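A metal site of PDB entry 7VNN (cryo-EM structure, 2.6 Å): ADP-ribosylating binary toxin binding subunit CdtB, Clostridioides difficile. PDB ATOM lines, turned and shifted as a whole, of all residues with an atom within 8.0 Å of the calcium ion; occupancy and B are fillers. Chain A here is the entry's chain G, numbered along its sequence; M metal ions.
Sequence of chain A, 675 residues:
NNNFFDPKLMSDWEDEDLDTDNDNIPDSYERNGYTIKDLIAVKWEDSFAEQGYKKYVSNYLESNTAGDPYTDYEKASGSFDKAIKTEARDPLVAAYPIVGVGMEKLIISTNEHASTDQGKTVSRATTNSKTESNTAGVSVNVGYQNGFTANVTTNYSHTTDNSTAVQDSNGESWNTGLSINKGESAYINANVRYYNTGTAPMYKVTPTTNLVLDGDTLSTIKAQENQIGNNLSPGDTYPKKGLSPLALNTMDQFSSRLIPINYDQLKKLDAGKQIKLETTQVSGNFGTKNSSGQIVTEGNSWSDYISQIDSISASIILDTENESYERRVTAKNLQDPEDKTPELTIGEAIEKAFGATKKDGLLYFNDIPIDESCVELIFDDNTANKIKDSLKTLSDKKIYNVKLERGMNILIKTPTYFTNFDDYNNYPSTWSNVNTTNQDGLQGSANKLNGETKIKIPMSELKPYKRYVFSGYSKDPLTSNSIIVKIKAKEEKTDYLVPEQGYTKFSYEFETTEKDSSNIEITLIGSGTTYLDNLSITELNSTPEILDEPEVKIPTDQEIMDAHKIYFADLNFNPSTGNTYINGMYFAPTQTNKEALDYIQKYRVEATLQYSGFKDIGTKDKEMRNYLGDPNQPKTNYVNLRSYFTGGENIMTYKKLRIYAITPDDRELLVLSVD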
ATOM      1  N   LEU A 362      -6.724 -33.817  20.838  1.00  0.00           N
ATOM      2  CA  LEU A 362      -8.044 -33.263  20.616  1.00  0.00           C
ATOM      3  C   LEU A 362      -8.945 -34.327  20.009  1.00  0.00           C
ATOM      4  O   LEU A 362      -8.524 -35.105  19.142  1.00  0.00           O
ATOM      5  CB  LEU A 362      -7.990 -32.043  19.701  1.00  0.00           C
ATOM      6  CG  LEU A 362      -6.911 -31.011  20.056  1.00  0.00           C
ATOM      7  CD1 LEU A 362      -6.915 -29.859  19.070  1.00  0.00           C
ATOM      8  CD2 LEU A 362      -7.103 -30.505  21.472  1.00  0.00           C
ATOM      9  N   PHE A 418     -17.218 -22.854  11.733  1.00  0.00           N
ATOM     10  CA  PHE A 418     -16.155 -22.779  12.709  1.00  0.00           C
ATOM     11  C   PHE A 418     -14.821 -22.585  11.994  1.00  0.00           C
ATOM     12  O   PHE A 418     -14.661 -22.979  10.841  1.00  0.00           O
ATOM     13  CB  PHE A 418     -16.119 -24.043  13.573  1.00  0.00           C
ATOM     14  CG  PHE A 418     -14.985 -24.084  14.569  1.00  0.00           C
ATOM     15  CD1 PHE A 418     -15.006 -23.269  15.694  1.00  0.00           C
ATOM     16  CD2 PHE A 418     -13.905 -24.928  14.374  1.00  0.00           C
ATOM     17  CE1 PHE A 418     -13.970 -23.305  16.598  1.00  0.00           C
ATOM     18  CE2 PHE A 418     -12.869 -24.964  15.278  1.00  0.00           C
ATOM     19  CZ  PHE A 418     -12.900 -24.149  16.394  1.00  0.00           C
ATOM     20  N   THR A 419     -13.873 -21.963  12.703  1.00  0.00           N
ATOM     21  CA  THR A 419     -12.528 -21.810  12.190  1.00  0.00           C
ATOM     22  C   THR A 419     -11.538 -21.768  13.350  1.00  0.00           C
ATOM     23  O   THR A 419     -11.810 -21.144  14.381  1.00  0.00           O
ATOM     24  CB  THR A 419     -12.380 -20.552  11.329  1.00  0.00           C
ATOM     25  OG1 THR A 419     -11.027 -20.435  10.860  1.00  0.00           O
ATOM     26  CG2 THR A 419     -12.748 -19.298  12.123  1.00  0.00           C
ATOM     27  N   ASN A 420     -10.415 -22.456  13.180  1.00  0.00           N
ATOM     28  CA  ASN A 420      -9.319 -22.416  14.132  1.00  0.00           C
ATOM     29  C   ASN A 420      -8.119 -21.651  13.615  1.00  0.00           C
ATOM     30  O   ASN A 420      -7.100 -21.559  14.311  1.00  0.00           O
ATOM     31  CB  ASN A 420      -8.895 -23.837  14.536  1.00  0.00           C
ATOM     32  CG  ASN A 420      -8.475 -24.667  13.338  1.00  0.00           C
ATOM     33  OD1 ASN A 420      -8.984 -24.505  12.239  1.00  0.00           O
ATOM     34  ND2 ASN A 420      -7.521 -25.570  13.555  1.00  0.00           N
ATOM     35  N   PHE A 421      -8.210 -21.104  12.395  1.00  0.00           N
ATOM     36  CA  PHE A 421      -7.149 -20.370  11.707  1.00  0.00           C
ATOM     37  C   PHE A 421      -5.928 -21.224  11.410  1.00  0.00           C
ATOM     38  O   PHE A 421      -4.868 -20.686  11.068  1.00  0.00           O
ATOM     39  CB  PHE A 421      -6.724 -19.112  12.481  1.00  0.00           C
ATOM     40  CG  PHE A 421      -7.850 -18.193  12.822  1.00  0.00           C
ATOM     41  CD1 PHE A 421      -8.600 -17.597  11.818  1.00  0.00           C
ATOM     42  CD2 PHE A 421      -8.158 -17.898  14.137  1.00  0.00           C
ATOM     43  CE1 PHE A 421      -9.633 -16.743  12.126  1.00  0.00           C
ATOM     44  CE2 PHE A 421      -9.198 -17.049  14.451  1.00  0.00           C
ATOM     45  CZ  PHE A 421      -9.935 -16.472  13.446  1.00  0.00           C
ATOM     46  N   ASP A 422      -6.031 -22.548  11.539  1.00  0.00           N
ATOM     47  CA  ASP A 422      -4.918 -23.425  11.152  1.00  0.00           C
ATOM     48  C   ASP A 422      -5.282 -24.350   9.996  1.00  0.00           C
ATOM     49  O   ASP A 422      -4.655 -24.283   8.944  1.00  0.00           O
ATOM     50  CB  ASP A 422      -4.466 -24.239  12.371  1.00  0.00           C
ATOM     51  CG  ASP A 422      -3.644 -23.426  13.335  1.00  0.00           C
ATOM     52  OD1 ASP A 422      -3.209 -22.318  12.962  1.00  0.00           O
ATOM     53  OD2 ASP A 422      -3.434 -23.903  14.471  1.00  0.00           O
ATOM     54  N   ASP A 423      -6.284 -25.213  10.173  1.00  0.00           N
ATOM     55  CA  ASP A 423      -6.643 -26.176   9.136  1.00  0.00           C
ATOM     56  C   ASP A 423      -8.135 -26.346   8.921  1.00  0.00           C
ATOM     57  O   ASP A 423      -8.527 -26.781   7.825  1.00  0.00           O
ATOM     58  CB  ASP A 423      -6.035 -27.544   9.461  1.00  0.00           C
ATOM     59  CG  ASP A 423      -6.301 -27.982  10.889  1.00  0.00           C
ATOM     60  OD1 ASP A 423      -6.872 -27.184  11.656  1.00  0.00           O
ATOM     61  OD2 ASP A 423      -5.934 -29.122  11.244  1.00  0.00           O
ATOM     62  N   TYR A 424      -8.986 -26.027   9.880  1.00  0.00           N
ATOM     63  CA  TYR A 424     -10.425 -26.258   9.784  1.00  0.00           C
ATOM     64  C   TYR A 424     -11.106 -24.932   9.484  1.00  0.00           C
ATOM     65  O   TYR A 424     -11.298 -24.099  10.378  1.00  0.00           O
ATOM     66  CB  TYR A 424     -10.963 -26.885  11.069  1.00  0.00           C
ATOM     67  CG  TYR A 424     -12.362 -27.441  10.929  1.00  0.00           C
ATOM     68  CD1 TYR A 424     -12.576 -28.727  10.434  1.00  0.00           C
ATOM     69  CD2 TYR A 424     -13.468 -26.677  11.261  1.00  0.00           C
ATOM     70  CE1 TYR A 424     -13.849 -29.232  10.296  1.00  0.00           C
ATOM     71  CE2 TYR A 424     -14.741 -27.182  11.123  1.00  0.00           C
ATOM     72  CZ  TYR A 424     -14.933 -28.450  10.646  1.00  0.00           C
ATOM     73  OH  TYR A 424     -16.203 -28.948  10.516  1.00  0.00           O
ATOM     74  N   THR A 436      -1.946 -15.884   9.842  1.00  0.00           N
ATOM     75  CA  THR A 436      -1.725 -16.957  10.798  1.00  0.00           C
ATOM     76  C   THR A 436      -0.256 -17.350  10.885  1.00  0.00           C
ATOM     77  O   THR A 436       0.066 -18.519  11.114  1.00  0.00           O
ATOM     78  CB  THR A 436      -2.584 -18.164  10.444  1.00  0.00           C
ATOM     79  OG1 THR A 436      -2.006 -18.844   9.315  1.00  0.00           O
ATOM     80  CG2 THR A 436      -3.995 -17.729  10.084  1.00  0.00           C
ATOM     81  N   GLN A 439       2.478 -17.819  16.403  1.00  0.00           N
ATOM     82  CA  GLN A 439       2.060 -18.941  17.233  1.00  0.00           C
ATOM     83  C   GLN A 439       1.406 -18.371  18.492  1.00  0.00           C
ATOM     84  O   GLN A 439       2.078 -18.118  19.488  1.00  0.00           O
ATOM     85  CB  GLN A 439       3.227 -19.863  17.566  1.00  0.00           C
ATOM     86  CG  GLN A 439       3.826 -20.555  16.356  1.00  0.00           C
ATOM     87  CD  GLN A 439       2.832 -21.483  15.689  1.00  0.00           C
ATOM     88  OE1 GLN A 439       2.359 -21.203  14.582  1.00  0.00           O
ATOM     89  NE2 GLN A 439       2.516 -22.597  16.345  1.00  0.00           N
ATOM     90  N   ASP A 440       0.093 -18.184  18.431  1.00  0.00           N
ATOM     91  CA  ASP A 440      -0.661 -17.633  19.549  1.00  0.00           C
ATOM     92  C   ASP A 440      -2.055 -18.275  19.527  1.00  0.00           C
ATOM     93  O   ASP A 440      -2.284 -19.258  18.820  1.00  0.00           O
ATOM     94  CB  ASP A 440      -0.714 -16.099  19.474  1.00  0.00           C
ATOM     95  CG  ASP A 440       0.521 -15.442  20.051  1.00  0.00           C
ATOM     96  OD1 ASP A 440       0.785 -15.617  21.258  1.00  0.00           O
ATOM     97  OD2 ASP A 440       1.238 -14.757  19.290  1.00  0.00           O
ATOM     98  N   GLY A 441      -2.979 -17.708  20.304  1.00  0.00           N
ATOM     99  CA  GLY A 441      -4.315 -18.257  20.371  1.00  0.00           C
ATOM    100  C   GLY A 441      -4.342 -19.555  21.150  1.00  0.00           C
ATOM    101  O   GLY A 441      -3.389 -19.951  21.822  1.00  0.00           O
ATOM    102  N   LEU A 442      -5.496 -20.237  21.055  1.00  0.00           N
ATOM    103  CA  LEU A 442      -5.661 -21.499  21.771  1.00  0.00           C
ATOM    104  C   LEU A 442      -4.665 -22.541  21.283  1.00  0.00           C
ATOM    105  O   LEU A 442      -4.057 -23.246  22.090  1.00  0.00           O
ATOM    106  CB  LEU A 442      -7.095 -22.007  21.615  1.00  0.00           C
ATOM    107  CG  LEU A 442      -8.179 -21.446  22.544  1.00  0.00           C
ATOM    108  CD1 LEU A 442      -7.879 -21.823  23.990  1.00  0.00           C
ATOM    109  CD2 LEU A 442      -8.314 -19.941  22.400  1.00  0.00           C
ATOM    110  N   GLN A 443      -4.497 -22.664  19.965  1.00  0.00           N
ATOM    111  CA  GLN A 443      -3.526 -23.586  19.378  1.00  0.00           C
ATOM    112  C   GLN A 443      -2.907 -22.920  18.152  1.00  0.00           C
ATOM    113  O   GLN A 443      -3.426 -23.063  17.039  1.00  0.00           O
ATOM    114  CB  GLN A 443      -4.176 -24.921  19.016  1.00  0.00           C
ATOM    115  CG  GLN A 443      -4.727 -25.705  20.196  1.00  0.00           C
ATOM    116  CD  GLN A 443      -6.221 -25.492  20.380  1.00  0.00           C
ATOM    117  OE1 GLN A 443      -6.909 -25.018  19.476  1.00  0.00           O
ATOM    118  NE2 GLN A 443      -6.728 -25.843  21.557  1.00  0.00           N
ATOM    119  N   GLY A 444      -1.821 -22.188  18.356  1.00  0.00           N
ATOM    120  CA  GLY A 444      -0.981 -21.742  17.241  1.00  0.00           C
ATOM    121  C   GLY A 444      -1.690 -20.936  16.172  1.00  0.00           C
ATOM    122  O   GLY A 444      -1.485 -21.199  14.980  1.00  0.00           O
ATOM    123  N   SER A 445      -2.509 -19.972  16.562  1.00  0.00           N
ATOM    124  CA  SER A 445      -3.256 -19.186  15.582  1.00  0.00           C
ATOM    125  C   SER A 445      -3.799 -17.892  16.170  1.00  0.00           C
ATOM    126  O   SER A 445      -4.458 -17.904  17.213  1.00  0.00           O
ATOM    127  CB  SER A 445      -4.398 -20.022  15.004  1.00  0.00           C
ATOM    128  OG  SER A 445      -5.289 -20.429  16.018  1.00  0.00           O
ATOM    129  N   ALA A 446      -3.551 -16.767  15.503  1.00  0.00           N
ATOM    130  CA  ALA A 446      -3.942 -15.457  16.016  1.00  0.00           C
ATOM    131  C   ALA A 446      -4.937 -14.736  15.108  1.00  0.00           C
ATOM    132  O   ALA A 446      -5.988 -14.304  15.593  1.00  0.00           O
ATOM    133  CB  ALA A 446      -2.699 -14.580  16.208  1.00  0.00           C
ATOM    134  N   LEU A 532      -7.288 -13.412  18.571  1.00  0.00           N
ATOM    135  CA  LEU A 532      -8.530 -14.121  18.325  1.00  0.00           C
ATOM    136  C   LEU A 532      -8.241 -15.577  17.999  1.00  0.00           C
ATOM    137  O   LEU A 532      -7.160 -15.905  17.491  1.00  0.00           O
ATOM    138  CB  LEU A 532      -9.327 -13.485  17.177  1.00  0.00           C
ATOM    139  CG  LEU A 532      -9.854 -12.065  17.433  1.00  0.00           C
ATOM    140  CD1 LEU A 532     -10.498 -11.505  16.181  1.00  0.00           C
ATOM    141  CD2 LEU A 532     -10.832 -12.058  18.598  1.00  0.00           C
ATOM    142  N   ASP A 533      -9.201 -16.446  18.305  1.00  0.00           N
ATOM    143  CA  ASP A 533      -9.090 -17.865  17.987  1.00  0.00           C
ATOM    144  C   ASP A 533     -10.445 -18.526  18.177  1.00  0.00           C
ATOM    145  O   ASP A 533     -11.218 -18.137  19.057  1.00  0.00           O
ATOM    146  CB  ASP A 533      -8.039 -18.549  18.868  1.00  0.00           C
ATOM    147  CG  ASP A 533      -7.287 -19.638  18.125  1.00  0.00           C
ATOM    148  OD1 ASP A 533      -7.676 -19.962  16.983  1.00  0.00           O
ATOM    149  OD2 ASP A 533      -6.315 -20.172  18.690  1.00  0.00           O
ATOM    150  N   ASN A 534     -10.708 -19.537  17.355  1.00  0.00           N
ATOM    151  CA  ASN A 534     -11.896 -20.377  17.459  1.00  0.00           C
ATOM    152  C   ASN A 534     -13.177 -19.550  17.354  1.00  0.00           C
ATOM    153  O   ASN A 534     -13.986 -19.467  18.286  1.00  0.00           O
ATOM    154  CB  ASN A 534     -11.875 -21.195  18.753  1.00  0.00           C
ATOM    155  CG  ASN A 534     -10.683 -22.139  18.831  1.00  0.00           C
ATOM    156  OD1 ASN A 534     -10.119 -22.519  17.801  1.00  0.00           O
ATOM    157  ND2 ASN A 534     -10.310 -22.526  20.032  1.00  0.00           N
HETATM  158 CA    CA M   1      -5.417 -22.814  15.741  1.00  0.00          CA
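Asp 533 touches the calcium ion (OD1 to CA, 3.8 Å). Five residues have an atom within 4 Å of the calcium ion: Asn 420, Asp 422, Gln 443, Ser 445 and Asp 533.
N of Gln 443 sits at hydrogen-bond distance from OD2 of Asp 533 (3.3 Å). OG of Ser 445 lies close to OD1 of Asp 533, at 2.6 Å. The side-chain amide nitrogen (ND2) of Asn 420 sits at hydrogen-bond distance from the side-chain carboxylate (OD1) of Asp 423 (2.6 Å). The side-chain amide oxygen (OD1) of Asn 420 sits at hydrogen-bond distance from the backbone NH (N) of Tyr 424. The side-chain carboxylate (OD2) of Asp 533 is in hydrogen-bond range of the backbone NH (N) of Leu 442 (2.5 Å).
The calcium ion is bound by O of Gln 443 (2.4 Å). The side-chain hydroxyl (OG) of Ser 445 binds the calcium ion (2.4 Å). O of Asn 420 binds the calcium ion (2.5 Å). OD2 of Asp 422 binds the calcium ion (2.6 Å).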
